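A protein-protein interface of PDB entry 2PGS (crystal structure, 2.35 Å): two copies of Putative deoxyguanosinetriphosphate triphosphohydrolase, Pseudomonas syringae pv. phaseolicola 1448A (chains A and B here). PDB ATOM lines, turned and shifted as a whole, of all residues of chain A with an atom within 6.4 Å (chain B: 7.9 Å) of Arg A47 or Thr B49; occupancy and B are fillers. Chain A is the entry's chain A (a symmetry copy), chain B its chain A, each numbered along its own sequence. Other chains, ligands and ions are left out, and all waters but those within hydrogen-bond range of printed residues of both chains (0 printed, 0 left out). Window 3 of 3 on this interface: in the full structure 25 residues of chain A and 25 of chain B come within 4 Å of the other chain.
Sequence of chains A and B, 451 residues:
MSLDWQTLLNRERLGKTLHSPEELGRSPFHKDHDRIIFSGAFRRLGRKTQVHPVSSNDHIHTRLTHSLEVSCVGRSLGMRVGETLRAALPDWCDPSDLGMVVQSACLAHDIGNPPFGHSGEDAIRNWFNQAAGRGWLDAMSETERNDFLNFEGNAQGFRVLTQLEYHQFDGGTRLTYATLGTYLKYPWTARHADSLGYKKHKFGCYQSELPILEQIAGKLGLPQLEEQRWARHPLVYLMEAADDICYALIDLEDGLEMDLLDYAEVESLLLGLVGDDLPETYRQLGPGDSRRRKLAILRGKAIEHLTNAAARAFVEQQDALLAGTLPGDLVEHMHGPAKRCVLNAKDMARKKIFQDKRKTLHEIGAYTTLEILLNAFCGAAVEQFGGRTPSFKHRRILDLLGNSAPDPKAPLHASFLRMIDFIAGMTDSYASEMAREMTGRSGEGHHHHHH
The guanidinium group (NH1) of Arg B47 lies close to the guanidinium group (NH1) of Arg A47, 2.6 Å away.
The backbone carbonyl oxygen of Leu B45 lies within hydrogen-bond range of the backbone NH of Leu B64 (3.3 Å).
The backbone carbonyl oxygen (O) of Arg B47 lies within hydrogen-bond range of the backbone NH (N) of Asp B428, at 3.2 Å.
The backbone NH (N) of Thr B62 sits at hydrogen-bond distance from the side-chain hydroxyl (OG1) of Thr B65 (3.0 Å).
N of Asp A428 is in hydrogen-bond range of O of Arg A47, 3.2 Å away.
The backbone NH of Thr A49 sits at hydrogen-bond distance from the side-chain carboxylate of Asp A428 (3.0 Å).
OG1 of Thr A62 sits close to N of Leu A64, at 3.1 Å.
Among the printed residues, merely in contact across the chains: Arg A43 with His B61 (3.8 Å), Gly A46 with Arg B47 (3.7 Å), Arg A47 with Gly B46 (3.7 Å), Arg A47 with Thr B49 (3.7 Å), Arg A47 with Thr B62 (3.3 Å), Thr A49 with Arg B47 (3.7 Å), Thr A62 with Arg B47 (3.3 Å) and Leu A64 with Leu B64 (3.9 Å).
Arg A47 touches just these residues of chain B: Gly B46, Arg B47, Thr B49 and Thr B62.
Of the printed residues of chain A, Thr B49 touches Arg A47.
Printed residues of chain B within 4 Å of Thr A62: Arg B47.
Printed residues of chain B within 4 Å of Arg A43: His B61.
Printed residues of chain A within 4 Å of Arg B47: Gly A46, Arg A47, Thr A49 and Thr A62.
Of the printed residues of chain A, Gly B46 touches Arg A47 (3.7 Å).
Of the printed residues of chain B, Leu A64 touches Leu B64 (3.9 Å).
The nearest residue of chain B that does not touch Arg A47 is Lys B48 (5.6 Å).
The nearest printed residue of chain B that does not touch Thr A49 is Gly B46 (9.2 Å).
Of the 25 printed residues of chain B, 6 touch a printed residue of chain A.
Hydrophobic or aromatic side chains of chain B within 4 Å of the printed part of chain A: His B61 and Leu B64.
Hydrophobic or aromatic side chains of chain A that line the printed part of chain B: Leu A64.
Gly A46 touches Arg B47, and with the chains exchanged Arg A47 touches Gly B46.
Arg A47 touches Thr B49, and with the chains exchanged Thr A49 touches Arg B47.
Arg A47 touches Thr B62, and with the chains exchanged Thr A62 touches Arg B47.
Leu B64 touches its own counterpart, Leu A64.
Positions printed for both chains: 44, 45, 46, 47, 48, 49, 62, 64, 427, 428 and 429.
Of the 9 pairs that touch across the chains among the printed residues, 8 have their exchanged pair printed and touching as well.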
ATOM      1  N   ARG A  43     -20.305  12.491   8.742  1.00  0.00           N
ATOM      2  CA  ARG A  43     -21.471  13.052   8.050  1.00  0.00           C
ATOM      3  C   ARG A  43     -22.777  12.493   8.608  1.00  0.00           C
ATOM      4  O   ARG A  43     -23.729  13.235   8.834  1.00  0.00           O
ATOM      5  CB  ARG A  43     -21.403  12.756   6.551  1.00  0.00           C
ATOM      6  CG  ARG A  43     -20.372  13.559   5.786  1.00  0.00           C
ATOM      7  CD  ARG A  43     -20.180  12.996   4.377  1.00  0.00           C
ATOM      8  NE  ARG A  43     -19.204  13.770   3.612  1.00  0.00           N
ATOM      9  CZ  ARG A  43     -18.430  13.258   2.659  1.00  0.00           C
ATOM     10  NH1 ARG A  43     -18.515  11.970   2.360  1.00  0.00           N
ATOM     11  NH2 ARG A  43     -17.572  14.030   2.003  1.00  0.00           N
ATOM     12  N   ARG A  44     -22.813  11.187   8.846  1.00  0.00           N
ATOM     13  CA  ARG A  44     -24.012  10.561   9.379  1.00  0.00           C
ATOM     14  C   ARG A  44     -24.477  11.112  10.726  1.00  0.00           C
ATOM     15  O   ARG A  44     -25.614  10.891  11.117  1.00  0.00           O
ATOM     16  CB  ARG A  44     -23.812   9.045   9.468  1.00  0.00           C
ATOM     17  CG  ARG A  44     -23.753   8.376   8.089  1.00  0.00           C
ATOM     18  CD  ARG A  44     -23.504   6.883   8.197  1.00  0.00           C
ATOM     19  NE  ARG A  44     -22.464   6.463   7.260  1.00  0.00           N
ATOM     20  CZ  ARG A  44     -21.374   5.783   7.611  1.00  0.00           C
ATOM     21  NH1 ARG A  44     -21.178   5.442   8.881  1.00  0.00           N
ATOM     22  NH2 ARG A  44     -20.476   5.442   6.694  1.00  0.00           N
ATOM     23  N   LEU A  45     -23.606  11.818  11.444  1.00  0.00           N
ATOM     24  CA  LEU A  45     -23.993  12.388  12.735  1.00  0.00           C
ATOM     25  C   LEU A  45     -25.072  13.449  12.521  1.00  0.00           C
ATOM     26  O   LEU A  45     -25.834  13.773  13.422  1.00  0.00           O
ATOM     27  CB  LEU A  45     -22.783  13.014  13.434  1.00  0.00           C
ATOM     28  CG  LEU A  45     -21.667  12.062  13.878  1.00  0.00           C
ATOM     29  CD1 LEU A  45     -20.560  12.876  14.515  1.00  0.00           C
ATOM     30  CD2 LEU A  45     -22.191  11.036  14.868  1.00  0.00           C
ATOM     31  N   GLY A  46     -25.130  13.988  11.310  1.00  0.00           N
ATOM     32  CA  GLY A  46     -26.135  14.982  11.009  1.00  0.00           C
ATOM     33  C   GLY A  46     -27.522  14.362  11.019  1.00  0.00           C
ATOM     34  O   GLY A  46     -28.522  15.071  11.107  1.00  0.00           O
ATOM     35  N   ARG A  47     -27.594  13.035  10.922  1.00  0.00           N
ATOM     36  CA  ARG A  47     -28.885  12.350  10.941  1.00  0.00           C
ATOM     37  C   ARG A  47     -28.955  11.444  12.156  1.00  0.00           C
ATOM     38  O   ARG A  47     -29.611  10.410  12.135  1.00  0.00           O
ATOM     39  CB  ARG A  47     -29.100  11.537   9.655  1.00  0.00           C
ATOM     40  CG  ARG A  47     -29.194  12.380   8.360  1.00  0.00           C
ATOM     41  CD  ARG A  47     -30.263  13.477   8.450  1.00  0.00           C
ATOM     42  NE  ARG A  47     -30.421  14.242   7.206  1.00  0.00           N
ATOM     43  CZ  ARG A  47     -31.170  15.344   7.079  1.00  0.00           C
ATOM     44  NH1 ARG A  47     -31.839  15.835   8.118  1.00  0.00           N
ATOM     45  NH2 ARG A  47     -31.264  15.961   5.906  1.00  0.00           N
ATOM     46  N   LYS A  48     -28.254  11.842  13.212  1.00  0.00           N
ATOM     47  CA  LYS A  48     -28.237  11.098  14.466  1.00  0.00           C
ATOM     48  C   LYS A  48     -28.470  12.069  15.605  1.00  0.00           C
ATOM     49  O   LYS A  48     -27.754  13.063  15.756  1.00  0.00           O
ATOM     50  CB  LYS A  48     -26.900  10.389  14.669  1.00  0.00           C
ATOM     51  CG  LYS A  48     -26.693   9.175  13.785  1.00  0.00           C
ATOM     52  CD  LYS A  48     -25.442   8.412  14.210  1.00  0.00           C
ATOM     53  CE  LYS A  48     -25.336   7.101  13.503  1.00  0.00           C
ATOM     54  NZ  LYS A  48     -24.368   6.207  14.168  1.00  0.00           N
ATOM     55  N   THR A  49     -29.468  11.766  16.419  1.00  0.00           N
ATOM     56  CA  THR A  49     -29.810  12.636  17.529  1.00  0.00           C
ATOM     57  C   THR A  49     -29.880  11.841  18.818  1.00  0.00           C
ATOM     58  O   THR A  49     -29.894  10.613  18.797  1.00  0.00           O
ATOM     59  CB  THR A  49     -31.214  13.288  17.300  1.00  0.00           C
ATOM     60  OG1 THR A  49     -31.288  13.833  15.976  1.00  0.00           O
ATOM     61  CG2 THR A  49     -31.458  14.424  18.291  1.00  0.00           C
ATOM     62  N   THR A  62     -28.592  18.131  16.635  1.00  0.00           N
ATOM     63  CA  THR A  62     -28.164  16.759  16.377  1.00  0.00           C
ATOM     64  C   THR A  62     -26.802  16.452  16.996  1.00  0.00           C
ATOM     65  O   THR A  62     -26.150  17.317  17.583  1.00  0.00           O
ATOM     66  CB  THR A  62     -28.027  16.499  14.863  1.00  0.00           C
ATOM     67  OG1 THR A  62     -26.950  17.300  14.353  1.00  0.00           O
ATOM     68  CG2 THR A  62     -29.328  16.855  14.117  1.00  0.00           C
ATOM     69  N   LEU A  64     -24.314  15.996  15.363  1.00  0.00           N
ATOM     70  CA  LEU A  64     -23.344  16.719  14.544  1.00  0.00           C
ATOM     71  C   LEU A  64     -23.163  18.165  15.030  1.00  0.00           C
ATOM     72  O   LEU A  64     -22.039  18.637  15.149  1.00  0.00           O
ATOM     73  CB  LEU A  64     -23.769  16.725  13.073  1.00  0.00           C
ATOM     74  CG  LEU A  64     -23.010  17.637  12.095  1.00  0.00           C
ATOM     75  CD1 LEU A  64     -21.513  17.369  12.134  1.00  0.00           C
ATOM     76  CD2 LEU A  64     -23.549  17.394  10.678  1.00  0.00           C
ATOM     77  N   MET A 426     -25.609   3.035  11.412  1.00  0.00           N
ATOM     78  CA  MET A 426     -26.879   3.519  10.857  1.00  0.00           C
ATOM     79  C   MET A 426     -27.373   4.847  11.416  1.00  0.00           C
ATOM     80  O   MET A 426     -27.155   5.170  12.581  1.00  0.00           O
ATOM     81  CB  MET A 426     -27.992   2.480  11.050  1.00  0.00           C
ATOM     82  CG  MET A 426     -27.782   1.166  10.305  1.00  0.00           C
ATOM     83  SD  MET A 426     -29.146  -0.139  10.755  1.00  0.00           S
ATOM     84  CE  MET A 426     -28.946  -0.174  12.654  1.00  0.00           C
ATOM     85  N   THR A 427     -28.051   5.611  10.568  1.00  0.00           N
ATOM     86  CA  THR A 427     -28.632   6.872  10.982  1.00  0.00           C
ATOM     87  C   THR A 427     -29.879   6.438  11.736  1.00  0.00           C
ATOM     88  O   THR A 427     -30.333   5.311  11.556  1.00  0.00           O
ATOM     89  CB  THR A 427     -29.046   7.713   9.766  1.00  0.00           C
ATOM     90  OG1 THR A 427     -29.982   6.967   8.977  1.00  0.00           O
ATOM     91  CG2 THR A 427     -27.819   8.073   8.920  1.00  0.00           C
ATOM     92  N   ASP A 428     -30.426   7.301  12.579  1.00  0.00           N
ATOM     93  CA  ASP A 428     -31.620   6.935  13.328  1.00  0.00           C
ATOM     94  C   ASP A 428     -32.770   6.491  12.417  1.00  0.00           C
ATOM     95  O   ASP A 428     -33.359   5.433  12.633  1.00  0.00           O
ATOM     96  CB  ASP A 428     -32.127   8.103  14.168  1.00  0.00           C
ATOM     97  CG  ASP A 428     -31.133   8.560  15.214  1.00  0.00           C
ATOM     98  OD1 ASP A 428     -30.077   7.919  15.369  1.00  0.00           O
ATOM     99  OD2 ASP A 428     -31.423   9.567  15.885  1.00  0.00           O
ATOM    100  N   SER A 429     -33.085   7.290  11.398  1.00  0.00           N
ATOM    101  CA  SER A 429     -34.207   6.964  10.530  1.00  0.00           C
ATOM    102  C   SER A 429     -33.972   5.724   9.698  1.00  0.00           C
ATOM    103  O   SER A 429     -34.902   4.985   9.420  1.00  0.00           O
ATOM    104  CB  SER A 429     -34.553   8.129   9.602  1.00  0.00           C
ATOM    105  OG  SER A 429     -33.640   8.199   8.528  1.00  0.00           O
ATOM    106  N   ARG B  44     -29.541  25.460  11.577  1.00  0.00           N
ATOM    107  CA  ARG B  44     -30.645  25.063  10.718  1.00  0.00           C
ATOM    108  C   ARG B  44     -30.227  24.491   9.364  1.00  0.00           C
ATOM    109  O   ARG B  44     -31.028  23.851   8.698  1.00  0.00           O
ATOM    110  CB  ARG B  44     -31.602  26.242  10.522  1.00  0.00           C
ATOM    111  CG  ARG B  44     -32.374  26.595  11.799  1.00  0.00           C
ATOM    112  CD  ARG B  44     -33.278  27.797  11.598  1.00  0.00           C
ATOM    113  NE  ARG B  44     -33.135  28.743  12.703  1.00  0.00           N
ATOM    114  CZ  ARG B  44     -32.848  30.034  12.547  1.00  0.00           C
ATOM    115  NH1 ARG B  44     -32.675  30.539  11.330  1.00  0.00           N
ATOM    116  NH2 ARG B  44     -32.735  30.825  13.608  1.00  0.00           N
ATOM    117  N   LEU B  45     -28.985  24.724   8.946  1.00  0.00           N
ATOM    118  CA  LEU B  45     -28.517  24.190   7.667  1.00  0.00           C
ATOM    119  C   LEU B  45     -28.486  22.663   7.732  1.00  0.00           C
ATOM    120  O   LEU B  45     -28.528  21.982   6.717  1.00  0.00           O
ATOM    121  CB  LEU B  45     -27.119  24.723   7.337  1.00  0.00           C
ATOM    122  CG  LEU B  45     -26.992  26.227   7.070  1.00  0.00           C
ATOM    123  CD1 LEU B  45     -25.539  26.550   6.797  1.00  0.00           C
ATOM    124  CD2 LEU B  45     -27.847  26.641   5.885  1.00  0.00           C
ATOM    125  N   GLY B  46     -28.412  22.132   8.945  1.00  0.00           N
ATOM    126  CA  GLY B  46     -28.402  20.696   9.105  1.00  0.00           C
ATOM    127  C   GLY B  46     -29.744  20.102   8.707  1.00  0.00           C
ATOM    128  O   GLY B  46     -29.849  18.903   8.462  1.00  0.00           O
ATOM    129  N   ARG B  47     -30.781  20.937   8.646  1.00  0.00           N
ATOM    130  CA  ARG B  47     -32.107  20.460   8.256  1.00  0.00           C
ATOM    131  C   ARG B  47     -32.530  21.147   6.972  1.00  0.00           C
ATOM    132  O   ARG B  47     -33.711  21.365   6.732  1.00  0.00           O
ATOM    133  CB  ARG B  47     -33.138  20.719   9.365  1.00  0.00           C
ATOM    134  CG  ARG B  47     -32.885  19.947  10.683  1.00  0.00           C
ATOM    135  CD  ARG B  47     -32.751  18.435  10.459  1.00  0.00           C
ATOM    136  NE  ARG B  47     -32.585  17.673  11.705  1.00  0.00           N
ATOM    137  CZ  ARG B  47     -32.291  16.368  11.768  1.00  0.00           C
ATOM    138  NH1 ARG B  47     -32.121  15.657  10.658  1.00  0.00           N
ATOM    139  NH2 ARG B  47     -32.175  15.762  12.944  1.00  0.00           N
ATOM    140  N   LYS B  48     -31.542  21.499   6.156  1.00  0.00           N
ATOM    141  CA  LYS B  48     -31.782  22.144   4.870  1.00  0.00           C
ATOM    142  C   LYS B  48     -30.957  21.436   3.814  1.00  0.00           C
ATOM    143  O   LYS B  48     -29.736  21.303   3.939  1.00  0.00           O
ATOM    144  CB  LYS B  48     -31.393  23.620   4.912  1.00  0.00           C
ATOM    145  CG  LYS B  48     -32.351  24.501   5.689  1.00  0.00           C
ATOM    146  CD  LYS B  48     -32.005  25.972   5.490  1.00  0.00           C
ATOM    147  CE  LYS B  48     -33.059  26.863   6.063  1.00  0.00           C
ATOM    148  NZ  LYS B  48     -32.933  28.242   5.553  1.00  0.00           N
ATOM    149  N   THR B  49     -31.629  20.997   2.763  1.00  0.00           N
ATOM    150  CA  THR B  49     -30.956  20.274   1.700  1.00  0.00           C
ATOM    151  C   THR B  49     -31.280  20.894   0.355  1.00  0.00           C
ATOM    152  O   THR B  49     -32.190  21.712   0.245  1.00  0.00           O
ATOM    153  CB  THR B  49     -31.436  18.786   1.662  1.00  0.00           C
ATOM    154  OG1 THR B  49     -31.394  18.226   2.982  1.00  0.00           O
ATOM    155  CG2 THR B  49     -30.531  17.942   0.764  1.00  0.00           C
ATOM    156  N   GLN B  50     -30.507  20.525  -0.659  1.00  0.00           N
ATOM    157  CA  GLN B  50     -30.786  20.968  -2.014  1.00  0.00           C
ATOM    158  C   GLN B  50     -31.906  20.006  -2.409  1.00  0.00           C
ATOM    159  O   GLN B  50     -32.111  18.991  -1.738  1.00  0.00           O
ATOM    160  CB  GLN B  50     -29.578  20.740  -2.923  1.00  0.00           C
ATOM    161  CG  GLN B  50     -28.415  21.663  -2.649  1.00  0.00           C
ATOM    162  CD  GLN B  50     -28.827  23.125  -2.659  1.00  0.00           C
ATOM    163  OE1 GLN B  50     -29.703  23.529  -3.425  1.00  0.00           O
ATOM    164  NE2 GLN B  50     -28.187  23.930  -1.817  1.00  0.00           N
ATOM    165  N   VAL B  51     -32.644  20.306  -3.470  1.00  0.00           N
ATOM    166  CA  VAL B  51     -33.713  19.404  -3.880  1.00  0.00           C
ATOM    167  C   VAL B  51     -33.086  18.271  -4.690  1.00  0.00           C
ATOM    168  O   VAL B  51     -32.463  18.512  -5.720  1.00  0.00           O
ATOM    169  CB  VAL B  51     -34.794  20.157  -4.698  1.00  0.00           C
ATOM    170  CG1 VAL B  51     -35.786  19.177  -5.304  1.00  0.00           C
ATOM    171  CG2 VAL B  51     -35.536  21.114  -3.791  1.00  0.00           C
ATOM    172  N   HIS B  52     -33.236  17.041  -4.199  1.00  0.00           N
ATOM    173  CA  HIS B  52     -32.662  15.860  -4.849  1.00  0.00           C
ATOM    174  C   HIS B  52     -33.700  14.966  -5.513  1.00  0.00           C
ATOM    175  O   HIS B  52     -34.878  14.999  -5.161  1.00  0.00           O
ATOM    176  CB  HIS B  52     -31.894  15.022  -3.826  1.00  0.00           C
ATOM    177  CG  HIS B  52     -30.760  15.750  -3.181  1.00  0.00           C
ATOM    178  ND1 HIS B  52     -29.635  16.140  -3.875  1.00  0.00           N
ATOM    179  CD2 HIS B  52     -30.592  16.193  -1.912  1.00  0.00           C
ATOM    180  CE1 HIS B  52     -28.823  16.793  -3.063  1.00  0.00           C
ATOM    181  NE2 HIS B  52     -29.381  16.840  -1.866  1.00  0.00           N
ATOM    182  N   HIS B  61     -26.244  14.176   2.975  1.00  0.00           N
ATOM    183  CA  HIS B  61     -25.629  15.336   2.334  1.00  0.00           C
ATOM    184  C   HIS B  61     -26.526  16.563   2.364  1.00  0.00           C
ATOM    185  O   HIS B  61     -27.320  16.788   1.453  1.00  0.00           O
ATOM    186  CB  HIS B  61     -25.254  15.007   0.894  1.00  0.00           C
ATOM    187  CG  HIS B  61     -23.834  14.567   0.738  1.00  0.00           C
ATOM    188  ND1 HIS B  61     -22.767  15.412   0.962  1.00  0.00           N
ATOM    189  CD2 HIS B  61     -23.301  13.360   0.427  1.00  0.00           C
ATOM    190  CE1 HIS B  61     -21.639  14.745   0.799  1.00  0.00           C
ATOM    191  NE2 HIS B  61     -21.936  13.498   0.475  1.00  0.00           N
ATOM    192  N   THR B  62     -26.371  17.358   3.418  1.00  0.00           N
ATOM    193  CA  THR B  62     -27.158  18.570   3.625  1.00  0.00           C
ATOM    194  C   THR B  62     -26.362  19.835   3.312  1.00  0.00           C
ATOM    195  O   THR B  62     -25.174  19.787   2.986  1.00  0.00           O
ATOM    196  CB  THR B  62     -27.612  18.689   5.094  1.00  0.00           C
ATOM    197  OG1 THR B  62     -26.455  18.881   5.922  1.00  0.00           O
ATOM    198  CG2 THR B  62     -28.362  17.422   5.549  1.00  0.00           C
ATOM    199  N   ARG B  63     -27.015  20.979   3.421  1.00  0.00           N
ATOM    200  CA  ARG B  63     -26.308  22.215   3.167  1.00  0.00           C
ATOM    201  C   ARG B  63     -25.274  22.424   4.274  1.00  0.00           C
ATOM    202  O   ARG B  63     -24.292  23.129   4.077  1.00  0.00           O
ATOM    203  CB  ARG B  63     -27.292  23.385   3.088  1.00  0.00           C
ATOM    204  CG  ARG B  63     -28.102  23.378   1.782  1.00  0.00           C
ATOM    205  CD  ARG B  63     -29.342  24.248   1.859  1.00  0.00           C
ATOM    206  NE  ARG B  63     -29.015  25.600   2.282  1.00  0.00           N
ATOM    207  CZ  ARG B  63     -29.903  26.578   2.430  1.00  0.00           C
ATOM    208  NH1 ARG B  63     -31.191  26.350   2.185  1.00  0.00           N
ATOM    209  NH2 ARG B  63     -29.503  27.784   2.831  1.00  0.00           N
ATOM    210  N   LEU B  64     -25.477  21.789   5.425  1.00  0.00           N
ATOM    211  CA  LEU B  64     -24.517  21.925   6.518  1.00  0.00           C
ATOM    212  C   LEU B  64     -23.231  21.130   6.241  1.00  0.00           C
ATOM    213  O   LEU B  64     -22.137  21.644   6.437  1.00  0.00           O
ATOM    214  CB  LEU B  64     -25.128  21.458   7.842  1.00  0.00           C
ATOM    215  CG  LEU B  64     -24.203  21.293   9.059  1.00  0.00           C
ATOM    216  CD1 LEU B  64     -23.428  22.572   9.342  1.00  0.00           C
ATOM    217  CD2 LEU B  64     -25.057  20.918  10.278  1.00  0.00           C
ATOM    218  N   THR B  65     -23.353  19.884   5.792  1.00  0.00           N
ATOM    219  CA  THR B  65     -22.153  19.100   5.522  1.00  0.00           C
ATOM    220  C   THR B  65     -21.425  19.708   4.335  1.00  0.00           C
ATOM    221  O   THR B  65     -20.200  19.695   4.282  1.00  0.00           O
ATOM    222  CB  THR B  65     -22.489  17.622   5.261  1.00  0.00           C
ATOM    223  OG1 THR B  65     -23.500  17.524   4.250  1.00  0.00           O
ATOM    224  CG2 THR B  65     -22.990  16.985   6.548  1.00  0.00           C
ATOM    225  N   ASP B 110     -23.690  30.043   2.732  1.00  0.00           N
ATOM    226  CA  ASP B 110     -25.022  29.595   2.321  1.00  0.00           C
ATOM    227  C   ASP B 110     -26.059  29.745   3.427  1.00  0.00           C
ATOM    228  O   ASP B 110     -27.144  29.187   3.354  1.00  0.00           O
ATOM    229  CB  ASP B 110     -24.924  28.120   1.870  1.00  0.00           C
ATOM    230  CG  ASP B 110     -26.241  27.564   1.316  1.00  0.00           C
ATOM    231  OD1 ASP B 110     -26.902  28.261   0.508  1.00  0.00           O
ATOM    232  OD2 ASP B 110     -26.602  26.418   1.686  1.00  0.00           O
ATOM    233  N   PRO B 114     -33.178  29.907   1.519  1.00  0.00           N
ATOM    234  CA  PRO B 114     -34.428  29.413   2.091  1.00  0.00           C
ATOM    235  C   PRO B 114     -34.583  27.911   1.953  1.00  0.00           C
ATOM    236  O   PRO B 114     -33.725  27.236   1.386  1.00  0.00           O
ATOM    237  CB  PRO B 114     -35.475  30.144   1.261  1.00  0.00           C
ATOM    238  CG  PRO B 114     -34.868  30.016  -0.132  1.00  0.00           C
ATOM    239  CD  PRO B 114     -33.395  30.396   0.141  1.00  0.00           C
ATOM    240  N   PRO B 115     -35.691  27.370   2.479  1.00  0.00           N
ATOM    241  CA  PRO B 115     -35.944  25.929   2.378  1.00  0.00           C
ATOM    242  C   PRO B 115     -35.855  25.561   0.891  1.00  0.00           C
ATOM    243  O   PRO B 115     -36.092  26.416   0.016  1.00  0.00           O
ATOM    244  CB  PRO B 115     -37.375  25.791   2.886  1.00  0.00           C
ATOM    245  CG  PRO B 115     -37.511  26.915   3.861  1.00  0.00           C
ATOM    246  CD  PRO B 115     -36.763  28.057   3.227  1.00  0.00           C
ATOM    247  N   PHE B 116     -35.521  24.299   0.618  1.00  0.00           N
ATOM    248  CA  PHE B 116     -35.402  23.787  -0.746  1.00  0.00           C
ATOM    249  C   PHE B 116     -34.229  24.398  -1.513  1.00  0.00           C
ATOM    250  O   PHE B 116     -34.143  24.302  -2.734  1.00  0.00           O
ATOM    251  CB  PHE B 116     -36.739  23.985  -1.473  1.00  0.00           C
ATOM    252  CG  PHE B 116     -37.921  23.529  -0.653  1.00  0.00           C
ATOM    253  CD1 PHE B 116     -37.976  22.224  -0.159  1.00  0.00           C
ATOM    254  CD2 PHE B 116     -38.916  24.428  -0.277  1.00  0.00           C
ATOM    255  CE1 PHE B 116     -39.003  21.825   0.711  1.00  0.00           C
ATOM    256  CE2 PHE B 116     -39.949  24.044   0.589  1.00  0.00           C
ATOM    257  CZ  PHE B 116     -39.988  22.737   1.090  1.00  0.00           C
ATOM    258  N   GLY B 117     -33.321  25.015  -0.763  1.00  0.00           N
ATOM    259  CA  GLY B 117     -32.113  25.603  -1.320  1.00  0.00           C
ATOM    260  C   GLY B 117     -32.202  26.451  -2.570  1.00  0.00           C
ATOM    261  O   GLY B 117     -32.989  27.388  -2.634  1.00  0.00           O
ATOM    262  N   HIS B 118     -31.371  26.125  -3.557  1.00  0.00           N
ATOM    263  CA  HIS B 118     -31.327  26.866  -4.814  1.00  0.00           C
ATOM    264  C   HIS B 118     -32.665  26.879  -5.518  1.00  0.00           C
ATOM    265  O   HIS B 118     -33.031  27.872  -6.146  1.00  0.00           O
ATOM    266  CB  HIS B 118     -30.254  26.282  -5.732  1.00  0.00           C
ATOM    267  CG  HIS B 118     -28.866  26.431  -5.191  1.00  0.00           C
ATOM    268  ND1 HIS B 118     -27.913  25.438  -5.292  1.00  0.00           N
ATOM    269  CD2 HIS B 118     -28.273  27.457  -4.535  1.00  0.00           C
ATOM    270  CE1 HIS B 118     -26.794  25.846  -4.717  1.00  0.00           C
ATOM    271  NE2 HIS B 118     -26.985  27.068  -4.250  1.00  0.00           N
ATOM    272  N   SER B 119     -33.395  25.776  -5.415  1.00  0.00           N
ATOM    273  CA  SER B 119     -34.701  25.692  -6.046  1.00  0.00           C
ATOM    274  C   SER B 119     -35.645  26.655  -5.337  1.00  0.00           C
ATOM    275  O   SER B 119     -36.416  27.363  -5.978  1.00  0.00           O
ATOM    276  CB  SER B 119     -35.243  24.266  -5.960  1.00  0.00           C
ATOM    277  OG  SER B 119     -34.361  23.349  -6.593  1.00  0.00           O
ATOM    278  N   GLY B 120     -35.580  26.686  -4.010  1.00  0.00           N
ATOM    279  CA  GLY B 120     -36.441  27.581  -3.259  1.00  0.00           C
ATOM    280  C   GLY B 120     -36.099  29.021  -3.581  1.00  0.00           C
ATOM    281  O   GLY B 120     -36.956  29.896  -3.579  1.00  0.00           O
ATOM    282  N   THR B 427     -36.576  25.584   8.113  1.00  0.00           N
ATOM    283  CA  THR B 427     -35.932  24.351   7.708  1.00  0.00           C
ATOM    284  C   THR B 427     -36.874  23.813   6.643  1.00  0.00           C
ATOM    285  O   THR B 427     -38.030  24.224   6.594  1.00  0.00           O
ATOM    286  CB  THR B 427     -35.868  23.355   8.874  1.00  0.00           C
ATOM    287  OG1 THR B 427     -37.198  23.095   9.342  1.00  0.00           O
ATOM    288  CG2 THR B 427     -35.015  23.919  10.016  1.00  0.00           C
ATOM    289  N   ASP B 428     -36.399  22.917   5.789  1.00  0.00           N
ATOM    290  CA  ASP B 428     -37.260  22.371   4.749  1.00  0.00           C
ATOM    291  C   ASP B 428     -38.535  21.738   5.315  1.00  0.00           C
ATOM    292  O   ASP B 428     -39.635  22.045   4.860  1.00  0.00           O
ATOM    293  CB  ASP B 428     -36.536  21.299   3.939  1.00  0.00           C
ATOM    294  CG  ASP B 428     -35.320  21.824   3.208  1.00  0.00           C
ATOM    295  OD1 ASP B 428     -35.073  23.044   3.238  1.00  0.00           O
ATOM    296  OD2 ASP B 428     -34.615  21.001   2.596  1.00  0.00           O
ATOM    297  N   SER B 429     -38.392  20.862   6.310  1.00  0.00           N
ATOM    298  CA  SER B 429     -39.553  20.174   6.854  1.00  0.00           C
ATOM    299  C   SER B 429     -40.501  21.097   7.585  1.00  0.00           C
ATOM    300  O   SER B 429     -41.703  20.889   7.560  1.00  0.00           O
ATOM    301  CB  SER B 429     -39.143  19.038   7.791  1.00  0.00           C
ATOM    302  OG  SER B 429     -38.754  19.545   9.050  1.00  0.00           O
